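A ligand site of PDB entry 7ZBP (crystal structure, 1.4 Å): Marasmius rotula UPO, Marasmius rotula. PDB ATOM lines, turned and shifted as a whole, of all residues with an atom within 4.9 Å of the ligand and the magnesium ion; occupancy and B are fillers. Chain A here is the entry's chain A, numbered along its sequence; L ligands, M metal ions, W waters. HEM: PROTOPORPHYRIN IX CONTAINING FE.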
ATOM      1  N   PRO A  20      18.707 -10.803  -3.540  1.00  0.00           N
ATOM      2  CA  PRO A  20      18.193 -10.069  -2.374  1.00  0.00           C
ATOM      3  C   PRO A  20      19.289  -9.437  -1.510  1.00  0.00           C
ATOM      4  O   PRO A  20      18.990  -8.858  -0.477  1.00  0.00           O
ATOM      5  CB  PRO A  20      17.457 -11.153  -1.628  1.00  0.00           C
ATOM      6  CG  PRO A  20      18.336 -12.383  -1.856  1.00  0.00           C
ATOM      7  CD  PRO A  20      18.737 -12.263  -3.296  1.00  0.00           C
ATOM      8  N   CYS A  21      20.549  -9.597  -1.906  1.00  0.00           N
ATOM      9  CA  CYS A  21      21.712  -9.217  -1.089  1.00  0.00           C
ATOM     10  C   CYS A  21      22.312  -7.947  -1.683  1.00  0.00           C
ATOM     11  O   CYS A  21      22.871  -7.991  -2.781  1.00  0.00           O
ATOM     12  CB  CYS A  21      22.781 -10.299  -1.082  1.00  0.00           C
ATOM     13  SG  CYS A  21      24.250  -9.700  -0.259  1.00  0.00           S
ATOM     14  N   PRO A  22      22.245  -6.794  -0.990  1.00  0.00           N
ATOM     15  CA  PRO A  22      22.891  -5.600  -1.515  1.00  0.00           C
ATOM     16  C   PRO A  22      24.417  -5.698  -1.603  1.00  0.00           C
ATOM     17  O   PRO A  22      25.040  -5.043  -2.440  1.00  0.00           O
ATOM     18  CB  PRO A  22      22.497  -4.517  -0.503  1.00  0.00           C
ATOM     19  CG  PRO A  22      22.243  -5.270   0.767  1.00  0.00           C
ATOM     20  CD  PRO A  22      21.636  -6.598   0.334  1.00  0.00           C
ATOM     21  N   GLY A  23      25.010  -6.523  -0.750  1.00  0.00           N
ATOM     22  CA  GLY A  23      26.493  -6.662  -0.753  1.00  0.00           C
ATOM     23  C   GLY A  23      26.957  -7.291  -2.048  1.00  0.00           C
ATOM     24  O   GLY A  23      27.830  -6.707  -2.714  1.00  0.00           O
ATOM     25  N   LEU A  24      26.367  -8.399  -2.439  1.00  0.00           N
ATOM     26  CA  LEU A  24      26.780  -9.071  -3.688  1.00  0.00           C
ATOM     27  C   LEU A  24      26.274  -8.283  -4.899  1.00  0.00           C
ATOM     28  O   LEU A  24      26.982  -8.208  -5.915  1.00  0.00           O
ATOM     29  CB  LEU A  24      26.259 -10.498  -3.726  1.00  0.00           C
ATOM     30  CG  LEU A  24      26.737 -11.427  -2.638  1.00  0.00           C
ATOM     31  CD1 LEU A  24      26.084 -12.788  -2.770  1.00  0.00           C
ATOM     32  CD2 LEU A  24      28.264 -11.554  -2.577  1.00  0.00           C
ATOM     33  N   LEU A  27      28.783  -5.530  -5.522  1.00  0.00           N
ATOM     34  CA  LEU A  27      30.000  -6.052  -6.144  1.00  0.00           C
ATOM     35  C   LEU A  27      29.782  -6.319  -7.619  1.00  0.00           C
ATOM     36  O   LEU A  27      30.693  -6.001  -8.399  1.00  0.00           O
ATOM     37  CB  LEU A  27      30.474  -7.300  -5.415  1.00  0.00           C
ATOM     38  CG  LEU A  27      30.965  -7.092  -3.999  1.00  0.00           C
ATOM     39  CD1 LEU A  27      31.142  -8.418  -3.281  1.00  0.00           C
ATOM     40  CD2 LEU A  27      32.239  -6.262  -3.952  1.00  0.00           C
ATOM     41  N   ILE A  45      33.425 -15.032  -5.000  1.00  0.00           N
ATOM     42  CA  ILE A  45      32.828 -14.188  -3.912  1.00  0.00           C
ATOM     43  C   ILE A  45      33.947 -13.788  -2.941  1.00  0.00           C
ATOM     44  O   ILE A  45      34.035 -12.626  -2.510  1.00  0.00           O
ATOM     45  CB  ILE A  45      31.672 -14.895  -3.213  1.00  0.00           C
ATOM     46  CG1 ILE A  45      30.457 -15.014  -4.146  1.00  0.00           C
ATOM     47  CG2 ILE A  45      31.324 -14.183  -1.905  1.00  0.00           C
ATOM     48  CD1 ILE A  45      29.404 -15.978  -3.663  1.00  0.00           C
ATOM     49  N   GLY A  49      34.753  -9.918  -2.410  1.00  0.00           N
ATOM     50  CA  GLY A  49      34.500  -9.298  -1.106  1.00  0.00           C
ATOM     51  C   GLY A  49      35.790  -8.805  -0.447  1.00  0.00           C
ATOM     52  O   GLY A  49      35.757  -7.761   0.234  1.00  0.00           O
ATOM     53  N   TYR A  53      35.547  -4.798  -0.288  1.00  0.00           N
ATOM     54  CA  TYR A  53      35.133  -4.420   1.083  1.00  0.00           C
ATOM     55  C   TYR A  53      36.147  -4.689   2.175  1.00  0.00           C
ATOM     56  O   TYR A  53      35.857  -4.358   3.323  1.00  0.00           O
ATOM     57  CB  TYR A  53      33.848  -5.188   1.435  1.00  0.00           C
ATOM     58  CG  TYR A  53      32.695  -5.014   0.470  1.00  0.00           C
ATOM     59  CD1 TYR A  53      32.281  -3.769   0.056  1.00  0.00           C
ATOM     60  CD2 TYR A  53      31.846  -6.057   0.202  1.00  0.00           C
ATOM     61  CE1 TYR A  53      31.165  -3.615  -0.735  1.00  0.00           C
ATOM     62  CE2 TYR A  53      30.695  -5.905  -0.547  1.00  0.00           C
ATOM     63  CZ  TYR A  53      30.320  -4.677  -1.013  1.00  0.00           C
ATOM     64  OH  TYR A  53      29.207  -4.559  -1.810  1.00  0.00           O
ATOM     65  N   VAL A  55      36.494  -7.685   3.308  1.00  0.00           N
ATOM     66  CA  VAL A  55      35.866  -8.799   4.027  1.00  0.00           C
ATOM     67  C   VAL A  55      36.698 -10.049   3.758  1.00  0.00           C
ATOM     68  O   VAL A  55      36.998 -10.317   2.601  1.00  0.00           O
ATOM     69  CB  VAL A  55      34.388  -8.951   3.638  1.00  0.00           C
ATOM     70  CG1 VAL A  55      33.768 -10.139   4.314  1.00  0.00           C
ATOM     71  CG2 VAL A  55      33.602  -7.675   4.014  1.00  0.00           C
ATOM     72  N   LEU A  60      33.112 -15.175   4.126  1.00  0.00           N
ATOM     73  CA  LEU A  60      32.576 -15.387   2.772  1.00  0.00           C
ATOM     74  C   LEU A  60      32.536 -16.876   2.394  1.00  0.00           C
ATOM     75  O   LEU A  60      31.662 -17.267   1.613  1.00  0.00           O
ATOM     76  CB  LEU A  60      33.394 -14.556   1.810  1.00  0.00           C
ATOM     77  CG  LEU A  60      33.300 -13.042   2.064  1.00  0.00           C
ATOM     78  CD1 LEU A  60      34.220 -12.323   1.135  1.00  0.00           C
ATOM     79  CD2 LEU A  60      31.883 -12.551   1.863  1.00  0.00           C
ATOM     80  N   ALA A  63      29.300 -18.159   4.484  1.00  0.00           N
ATOM     81  CA  ALA A  63      28.065 -17.727   3.832  1.00  0.00           C
ATOM     82  C   ALA A  63      27.979 -18.258   2.409  1.00  0.00           C
ATOM     83  O   ALA A  63      26.893 -18.654   1.961  1.00  0.00           O
ATOM     84  CB  ALA A  63      27.999 -16.221   3.847  1.00  0.00           C
ATOM     85  N   GLY A  64      29.096 -18.186   1.685  1.00  0.00           N
ATOM     86  CA  GLY A  64      29.088 -18.530   0.262  1.00  0.00           C
ATOM     87  C   GLY A  64      28.650 -19.961   0.040  1.00  0.00           C
ATOM     88  O   GLY A  64      27.859 -20.209  -0.873  1.00  0.00           O
ATOM     89  N   GLY A  67      25.038 -20.282   0.425  1.00  0.00           N
ATOM     90  CA  GLY A  67      24.357 -19.744  -0.753  1.00  0.00           C
ATOM     91  C   GLY A  67      24.387 -20.685  -1.948  1.00  0.00           C
ATOM     92  O   GLY A  67      23.469 -20.701  -2.776  1.00  0.00           O
ATOM     93  N   LEU A  82      19.669 -16.707  -4.974  1.00  0.00           N
ATOM     94  CA  LEU A  82      19.756 -16.494  -3.522  1.00  0.00           C
ATOM     95  C   LEU A  82      18.441 -16.024  -2.936  1.00  0.00           C
ATOM     96  O   LEU A  82      18.323 -16.037  -1.722  1.00  0.00           O
ATOM     97  CB  LEU A  82      20.850 -15.458  -3.258  1.00  0.00           C
ATOM     98  CG  LEU A  82      22.286 -15.922  -3.451  1.00  0.00           C
ATOM     99  CD1 LEU A  82      23.225 -14.733  -3.351  1.00  0.00           C
ATOM    100  CD2 LEU A  82      22.694 -17.025  -2.501  1.00  0.00           C
ATOM    101  N   ILE A  88      19.121 -18.913   2.997  1.00  0.00           N
ATOM    102  CA  ILE A  88      19.506 -17.677   3.712  1.00  0.00           C
ATOM    103  C   ILE A  88      18.331 -16.686   3.713  1.00  0.00           C
ATOM    104  O   ILE A  88      18.078 -16.122   4.794  1.00  0.00           O
ATOM    105  CB  ILE A  88      20.765 -17.060   3.080  1.00  0.00           C
ATOM    106  CG1 ILE A  88      21.966 -18.002   3.183  1.00  0.00           C
ATOM    107  CG2 ILE A  88      21.074 -15.726   3.712  1.00  0.00           C
ATOM    108  CD1 ILE A  88      23.165 -17.546   2.353  1.00  0.00           C
ATOM    109  N   GLU A  89      17.652 -16.502   2.587  1.00  0.00           N
ATOM    110  CA  GLU A  89      16.595 -15.487   2.454  1.00  0.00           C
ATOM    111  C   GLU A  89      15.569 -15.739   3.554  1.00  0.00           C
ATOM    112  O   GLU A  89      15.126 -16.888   3.765  1.00  0.00           O
ATOM    113  CB  GLU A  89      15.984 -15.466   1.050  1.00  0.00           C
ATOM    114  CG  GLU A  89      15.132 -14.222   0.791  1.00  0.00           C
ATOM    115  CD  GLU A  89      13.765 -14.266   1.422  1.00  0.00           C
ATOM    116  OE1 GLU A  89      13.178 -15.329   1.371  1.00  0.00           O
ATOM    117  OE2 GLU A  89      13.330 -13.208   1.949  1.00  0.00           O
ATOM    118  N   HIS A  90      15.122 -14.665   4.188  1.00  0.00           N
ATOM    119  CA  HIS A  90      14.260 -14.723   5.392  1.00  0.00           C
ATOM    120  C   HIS A  90      13.230 -13.591   5.349  1.00  0.00           C
ATOM    121  O   HIS A  90      13.392 -12.567   4.712  1.00  0.00           O
ATOM    122  CB  HIS A  90      15.126 -14.651   6.669  1.00  0.00           C
ATOM    123  CG  HIS A  90      16.036 -13.492   6.644  1.00  0.00           C
ATOM    124  ND1 HIS A  90      15.558 -12.168   6.852  1.00  0.00           N
ATOM    125  CD2 HIS A  90      17.367 -13.376   6.396  1.00  0.00           C
ATOM    126  CE1 HIS A  90      16.587 -11.337   6.669  1.00  0.00           C
ATOM    127  NE2 HIS A  90      17.720 -12.048   6.423  1.00  0.00           N
ATOM    128  N   ASP A  91      12.186 -13.791   6.115  1.00  0.00           N
ATOM    129  CA  ASP A  91      11.253 -12.705   6.439  1.00  0.00           C
ATOM    130  C   ASP A  91      11.925 -11.642   7.289  1.00  0.00           C
ATOM    131  O   ASP A  91      13.006 -11.821   7.892  1.00  0.00           O
ATOM    132  CB  ASP A  91      10.085 -13.318   7.191  1.00  0.00           C
ATOM    133  CG  ASP A  91       9.379 -14.400   6.386  1.00  0.00           C
ATOM    134  OD1 ASP A  91       9.351 -14.295   5.145  1.00  0.00           O
ATOM    135  OD2 ASP A  91       8.799 -15.290   7.059  1.00  0.00           O
ATOM    136  N   SER A  93      13.202  -8.747   6.356  1.00  0.00           N
ATOM    137  CA  SER A  93      14.339  -8.071   5.710  1.00  0.00           C
ATOM    138  C   SER A  93      14.269  -6.556   5.941  1.00  0.00           C
ATOM    139  O   SER A  93      13.155  -6.022   6.192  1.00  0.00           O
ATOM    140  CB  SER A  93      14.384  -8.365   4.219  1.00  0.00           C
ATOM    141  OG  SER A  93      14.676  -9.750   4.039  1.00  0.00           O
ATOM    142  N   LEU A  94      15.411  -5.899   5.762  1.00  0.00           N
ATOM    143  CA  LEU A  94      15.507  -4.429   5.934  1.00  0.00           C
ATOM    144  C   LEU A  94      14.939  -3.711   4.725  1.00  0.00           C
ATOM    145  O   LEU A  94      14.598  -2.515   4.837  1.00  0.00           O
ATOM    146  CB  LEU A  94      16.962  -4.070   6.122  1.00  0.00           C
ATOM    147  CG  LEU A  94      17.613  -4.691   7.353  1.00  0.00           C
ATOM    148  CD1 LEU A  94      19.111  -4.539   7.332  1.00  0.00           C
ATOM    149  CD2 LEU A  94      17.071  -4.137   8.646  1.00  0.00           C
ATOM    150  N   SER A  95      14.993  -4.299   3.532  1.00  0.00           N
ATOM    151  CA  SER A  95      14.714  -3.582   2.288  1.00  0.00           C
ATOM    152  C   SER A  95      13.872  -4.379   1.305  1.00  0.00           C
ATOM    153  O   SER A  95      13.673  -3.857   0.187  1.00  0.00           O
ATOM    154  CB  SER A  95      15.983  -3.074   1.696  1.00  0.00           C
ATOM    155  OG  SER A  95      16.765  -4.166   1.182  1.00  0.00           O
ATOM    156  N   ARG A  96      13.431  -5.575   1.669  1.00  0.00           N
ATOM    157  CA  ARG A  96      12.628  -6.435   0.788  1.00  0.00           C
ATOM    158  C   ARG A  96      11.369  -6.813   1.553  1.00  0.00           C
ATOM    159  O   ARG A  96      11.370  -6.805   2.770  1.00  0.00           O
ATOM    160  CB  ARG A  96      13.397  -7.708   0.398  1.00  0.00           C
ATOM    161  CG  ARG A  96      14.304  -7.655  -0.829  1.00  0.00           C
ATOM    162  CD  ARG A  96      15.424  -6.650  -0.777  1.00  0.00           C
ATOM    163  NE  ARG A  96      16.281  -6.779  -1.943  1.00  0.00           N
ATOM    164  CZ  ARG A  96      17.266  -5.951  -2.231  1.00  0.00           C
ATOM    165  NH1 ARG A  96      17.592  -4.958  -1.417  1.00  0.00           N
ATOM    166  NH2 ARG A  96      17.982  -6.156  -3.321  1.00  0.00           N
ATOM    167  N   GLU A  97      10.334  -7.257   0.814  1.00  0.00           N
ATOM    168  CA  GLU A  97       9.094  -7.767   1.399  1.00  0.00           C
ATOM    169  C   GLU A  97       9.233  -9.243   1.720  1.00  0.00           C
ATOM    170  O   GLU A  97      10.073  -9.925   1.109  1.00  0.00           O
ATOM    171  CB  GLU A  97       7.917  -7.534   0.436  1.00  0.00           C
ATOM    172  CG  GLU A  97       7.696  -6.096   0.090  1.00  0.00           C
ATOM    173  CD  GLU A  97       6.652  -5.833  -0.973  1.00  0.00           C
ATOM    174  OE1 GLU A  97       6.518  -6.639  -1.893  1.00  0.00           O
ATOM    175  OE2 GLU A  97       5.915  -4.828  -0.827  1.00  0.00           O
ATOM    176  N   ASN A 104      10.255 -10.766  -2.450  1.00  0.00           N
ATOM    177  CA  ASN A 104      11.394 -10.990  -1.532  1.00  0.00           C
ATOM    178  C   ASN A 104      12.751 -10.731  -2.210  1.00  0.00           C
ATOM    179  O   ASN A 104      13.767 -11.020  -1.574  1.00  0.00           O
ATOM    180  CB  ASN A 104      11.351 -12.378  -0.909  1.00  0.00           C
ATOM    181  CG  ASN A 104      11.817 -13.460  -1.852  1.00  0.00           C
ATOM    182  OD1 ASN A 104      11.789 -13.277  -3.088  1.00  0.00           O
ATOM    183  ND2 ASN A 104      12.224 -14.591  -1.306  1.00  0.00           N
ATOM    184  N   GLU A 161      23.651  -9.553   8.965  1.00  0.00           N
ATOM    185  CA  GLU A 161      23.467  -8.679   7.808  1.00  0.00           C
ATOM    186  C   GLU A 161      23.537  -7.221   8.270  1.00  0.00           C
ATOM    187  O   GLU A 161      24.140  -6.416   7.593  1.00  0.00           O
ATOM    188  CB  GLU A 161      22.146  -9.029   7.094  1.00  0.00           C
ATOM    189  CG  GLU A 161      22.274 -10.361   6.367  1.00  0.00           C
ATOM    190  CD  GLU A 161      21.002 -11.085   5.996  1.00  0.00           C
ATOM    191  OE1 GLU A 161      19.934 -10.646   6.426  1.00  0.00           O
ATOM    192  OE2 GLU A 161      21.090 -12.160   5.377  1.00  0.00           O
ATOM    193  N   PHE A 164      27.113  -6.552   8.793  1.00  0.00           N
ATOM    194  CA  PHE A 164      27.800  -6.398   7.491  1.00  0.00           C
ATOM    195  C   PHE A 164      27.663  -4.957   7.027  1.00  0.00           C
ATOM    196  O   PHE A 164      28.665  -4.388   6.594  1.00  0.00           O
ATOM    197  CB  PHE A 164      27.242  -7.348   6.426  1.00  0.00           C
ATOM    198  CG  PHE A 164      27.706  -8.777   6.485  1.00  0.00           C
ATOM    199  CD1 PHE A 164      28.339  -9.298   7.599  1.00  0.00           C
ATOM    200  CD2 PHE A 164      27.238  -9.678   5.553  1.00  0.00           C
ATOM    201  CE1 PHE A 164      28.638 -10.649   7.680  1.00  0.00           C
ATOM    202  CE2 PHE A 164      27.583 -11.017   5.609  1.00  0.00           C
ATOM    203  CZ  PHE A 164      28.246 -11.516   6.689  1.00  0.00           C
ATOM    204  N   PHE A 165      26.466  -4.387   6.949  1.00  0.00           N
ATOM    205  CA  PHE A 165      26.372  -3.017   6.400  1.00  0.00           C
ATOM    206  C   PHE A 165      27.046  -2.017   7.347  1.00  0.00           C
ATOM    207  O   PHE A 165      27.693  -1.091   6.810  1.00  0.00           O
ATOM    208  CB  PHE A 165      24.941  -2.642   5.999  1.00  0.00           C
ATOM    209  CG  PHE A 165      24.021  -2.099   7.052  1.00  0.00           C
ATOM    210  CD1 PHE A 165      24.244  -0.843   7.613  1.00  0.00           C
ATOM    211  CD2 PHE A 165      22.916  -2.829   7.493  1.00  0.00           C
ATOM    212  CE1 PHE A 165      23.393  -0.372   8.605  1.00  0.00           C
ATOM    213  CE2 PHE A 165      22.048  -2.355   8.471  1.00  0.00           C
ATOM    214  CZ  PHE A 165      22.307  -1.106   8.999  1.00  0.00           C
ATOM    215  N   VAL A 168      31.021  -2.707   6.630  1.00  0.00           N
ATOM    216  CA  VAL A 168      31.554  -2.497   5.266  1.00  0.00           C
ATOM    217  C   VAL A 168      31.383  -1.041   4.841  1.00  0.00           C
ATOM    218  O   VAL A 168      32.242  -0.532   4.065  1.00  0.00           O
ATOM    219  CB  VAL A 168      30.898  -3.483   4.299  1.00  0.00           C
ATOM    220  CG1 VAL A 168      31.051  -3.113   2.871  1.00  0.00           C
ATOM    221  CG2 VAL A 168      31.334  -4.922   4.601  1.00  0.00           C
ATOM    222  N   PHE A 187      24.208   2.528  -0.667  1.00  0.00           N
ATOM    223  CA  PHE A 187      24.439   1.072  -0.737  1.00  0.00           C
ATOM    224  C   PHE A 187      23.120   0.354  -0.996  1.00  0.00           C
ATOM    225  O   PHE A 187      23.027  -0.515  -1.875  1.00  0.00           O
ATOM    226  CB  PHE A 187      25.132   0.662   0.554  1.00  0.00           C
ATOM    227  CG  PHE A 187      25.434  -0.813   0.722  1.00  0.00           C
ATOM    228  CD1 PHE A 187      26.354  -1.462  -0.097  1.00  0.00           C
ATOM    229  CD2 PHE A 187      24.758  -1.527   1.668  1.00  0.00           C
ATOM    230  CE1 PHE A 187      26.607  -2.817   0.106  1.00  0.00           C
ATOM    231  CE2 PHE A 187      25.021  -2.863   1.878  1.00  0.00           C
ATOM    232  CZ  PHE A 187      25.940  -3.513   1.088  1.00  0.00           C
ATOM    233  N   PHE A 188      22.071   0.620  -0.222  1.00  0.00           N
ATOM    234  CA  PHE A 188      20.779  -0.058  -0.367  1.00  0.00           C
ATOM    235  C   PHE A 188      20.048   0.430  -1.626  1.00  0.00           C
ATOM    236  O   PHE A 188      19.562  -0.385  -2.392  1.00  0.00           O
ATOM    237  CB  PHE A 188      19.928   0.117   0.883  1.00  0.00           C
ATOM    238  CG  PHE A 188      20.235  -0.850   2.000  1.00  0.00           C
ATOM    239  CD1 PHE A 188      19.585  -2.087   2.078  1.00  0.00           C
ATOM    240  CD2 PHE A 188      21.088  -0.508   3.035  1.00  0.00           C
ATOM    241  CE1 PHE A 188      19.825  -2.937   3.149  1.00  0.00           C
ATOM    242  CE2 PHE A 188      21.342  -1.377   4.076  1.00  0.00           C
ATOM    243  CZ  PHE A 188      20.712  -2.593   4.142  1.00  0.00           C
HETATM  244  CHA HEM L   1      21.022 -10.012   2.654  1.00  0.00           C
HETATM  245  CHB HEM L   1      25.151  -7.474   3.133  1.00  0.00           C
HETATM  246  CHC HEM L   1      27.646 -11.286   1.424  1.00  0.00           C
HETATM  247  CHD HEM L   1      23.487 -13.734   0.810  1.00  0.00           C
HETATM  248  C1A HEM L   1      21.908  -9.057   3.020  1.00  0.00           C
HETATM  249  C2A HEM L   1      21.606  -7.835   3.676  1.00  0.00           C
HETATM  250  C3A HEM L   1      22.781  -7.128   3.838  1.00  0.00           C
HETATM  251  C4A HEM L   1      23.827  -7.901   3.236  1.00  0.00           C
HETATM  252  CMA HEM L   1      22.981  -5.736   4.484  1.00  0.00           C
HETATM  253  CAA HEM L   1      20.232  -7.495   4.195  1.00  0.00           C
HETATM  254  CBA HEM L   1      19.230  -7.004   3.189  1.00  0.00           C
HETATM  255  CGA HEM L   1      17.916  -6.724   3.769  1.00  0.00           C
HETATM  256  O1A HEM L   1      17.115  -6.074   3.014  1.00  0.00           O
HETATM  257  O2A HEM L   1      17.620  -7.136   4.880  1.00  0.00           O
HETATM  258  C1B HEM L   1      26.176  -8.277   2.614  1.00  0.00           C
HETATM  259  C2B HEM L   1      27.551  -7.850   2.542  1.00  0.00           C
HETATM  260  C3B HEM L   1      28.226  -8.938   2.069  1.00  0.00           C
HETATM  261  C4B HEM L   1      27.294 -10.035   1.839  1.00  0.00           C
HETATM  262  CMB HEM L   1      28.160  -6.505   2.882  1.00  0.00           C
HETATM  263  CAB HEM L   1      29.677  -8.946   1.741  1.00  0.00           C
HETATM  264  CBB HEM L   1      30.096  -9.565   0.671  1.00  0.00           C
HETATM  265  C1C HEM L   1      26.777 -12.308   1.228  1.00  0.00           C
HETATM  266  C2C HEM L   1      27.107 -13.638   0.800  1.00  0.00           C
HETATM  267  C3C HEM L   1      25.927 -14.350   0.615  1.00  0.00           C
HETATM  268  C4C HEM L   1      24.844 -13.400   0.888  1.00  0.00           C
HETATM  269  CMC HEM L   1      28.533 -14.199   0.594  1.00  0.00           C
HETATM  270  CAC HEM L   1      25.692 -15.693   0.061  1.00  0.00           C
HETATM  271  CBC HEM L   1      26.484 -16.261  -0.839  1.00  0.00           C
HETATM  272  C1D HEM L   1      22.470 -12.875   1.252  1.00  0.00           C
HETATM  273  C2D HEM L   1      21.059 -13.274   1.109  1.00  0.00           C
HETATM  274  C3D HEM L   1      20.375 -12.207   1.653  1.00  0.00           C
HETATM  275  C4D HEM L   1      21.385 -11.226   2.046  1.00  0.00           C
HETATM  276  CMD HEM L   1      20.444 -14.526   0.582  1.00  0.00           C
HETATM  277  CAD HEM L   1      18.878 -12.019   1.815  1.00  0.00           C
HETATM  278  CBD HEM L   1      18.462 -12.172   3.265  1.00  0.00           C
HETATM  279  CGD HEM L   1      17.148 -11.482   3.450  1.00  0.00           C
HETATM  280  O1D HEM L   1      16.054 -12.144   3.381  1.00  0.00           O
HETATM  281  O2D HEM L   1      17.200 -10.258   3.659  1.00  0.00           O
HETATM  282  NA  HEM L   1      23.290  -9.088   2.750  1.00  0.00           N
HETATM  283  NB  HEM L   1      26.060  -9.566   2.223  1.00  0.00           N
HETATM  284  NC  HEM L   1      25.404 -12.229   1.354  1.00  0.00           N
HETATM  285  ND  HEM L   1      22.670 -11.645   1.742  1.00  0.00           N
HETATM  286 FE   HEM L   1      24.320 -10.612   1.928  1.00  0.00          FE
HETATM  287 MG    MG M   1      14.041 -11.530   2.934  1.00  0.00          MG
HETATM  288  O   HOH W   1      14.688 -10.773   1.023  1.00  0.00           O
HETATM  289  O   HOH W   2      18.241  -8.618   7.074  1.00  0.00           O
HETATM  290  O   HOH W   3      16.794  -8.963   1.142  1.00  0.00           O
HETATM  291  O   HOH W   4      12.168 -10.640   2.853  1.00  0.00           O
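An oxygen (O2A) of the ligand is in hydrogen-bond range of the backbone NH (N) of Leu 94, 2.7 Å away. The side-chain hydroxyl (OG) of Ser 95 lies within hydrogen-bond range of an oxygen (O1A) of the ligand, 2.7 Å away. O1A of the ligand is in hydrogen-bond range of N of Ser 95 (2.8 Å). The backbone NH of His 90 lies close to an oxygen (O1D) of the ligand, 2.8 Å away. An oxygen (O2D) of the ligand lies close to a ring nitrogen (NE2) of His 90, 3.3 Å away. SG of Cys 21 is bound to FE of the ligand (2.4 Å).
O of Gly 23 sits at hydrogen-bond distance from OH of Tyr 53 (2.7 Å). OE1 of Glu 161 lies within hydrogen-bond range of NE2 of His 90 (2.6 Å). The backbone NH (N) of Gly 23 sits close to the side-chain sulfur (SG) of Cys 21, 3.3 Å away. The side-chain carboxylate (OE1) of Glu 89 sits at hydrogen-bond distance from the side-chain amide nitrogen (ND2) of Asn 104 (2.9 Å). The side-chain hydroxyl (OG) of Ser 95 sits at hydrogen-bond distance from the guanidinium group (NH1) of Arg 96, at 2.8 Å. The side-chain sulfur (SG) of Cys 21 sits close to the backbone NH (N) of Leu 24 (3.3 Å).
Pro 20 touches the ligand (CG to CAD, 3.7 Å). CD of Pro 22 touches C2A of the ligand, at 3.6 Å. CA of Gly 23 touches C2B of the ligand, at 3.7 Å. Leu 24 touches the ligand. Ile 45 touches the ligand (CG2 to CMC, 3.7 Å). Tyr 53 touches the ligand (CE2 to CBB, 3.9 Å). Leu 60 touches the ligand (CD2 to CBB, 3.7 Å). O of Ala 63 touches CBC of the ligand (3.7 Å). CA of Gly 64 touches CBC of the ligand (3.6 Å). Leu 82 touches the ligand (O to CMD, 3.5 Å). Ile 88 touches the ligand. N of Arg 96 touches O1A of the ligand, at 3.95 Å. Glu 161 touches the ligand (OE2 to CBD, 3.4 Å). Phe 164 touches the ligand (CD2 to C1B, 3.4 Å). Phe 165 touches the ligand. Val 168 touches the ligand. CZ of Phe 188 touches CMA of the ligand, 3.9 Å away. Hydrophobic or aromatic side chains that line the ligand: Pro 20, Pro 22, Leu 24, Ile 45, Tyr 53, Leu 60, Ala 63, Leu 82, Ile 88, His 90, Leu 94, Phe 164, Phe 165, Val 168 and Phe 188. Of the 31 residues printed, 23 come within 4 Å of the ligand.
Of the 31 residues printed, 3 come within 4 Å of the magnesium ion. Along chain A the residues within 4 Å of the magnesium ion span positions 89 to 93.
The magnesium ion is bound by OE2 of Glu 89 (2.1 Å), water W4 (2.1 Å), O1D of the ligand (2.2 Å), water W1 (2.2 Å), O of His 90 (2.2 Å) and OG of Ser 93 (2.2 Å).
Water W2 bridges an oxygen (O2A) of the ligand (2.7 Å) and the side-chain carboxylate of Glu 161 (2.7 Å). Water W3 bridges O of Pro 20 (2.7 Å) and O2D of the ligand (2.9 Å).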
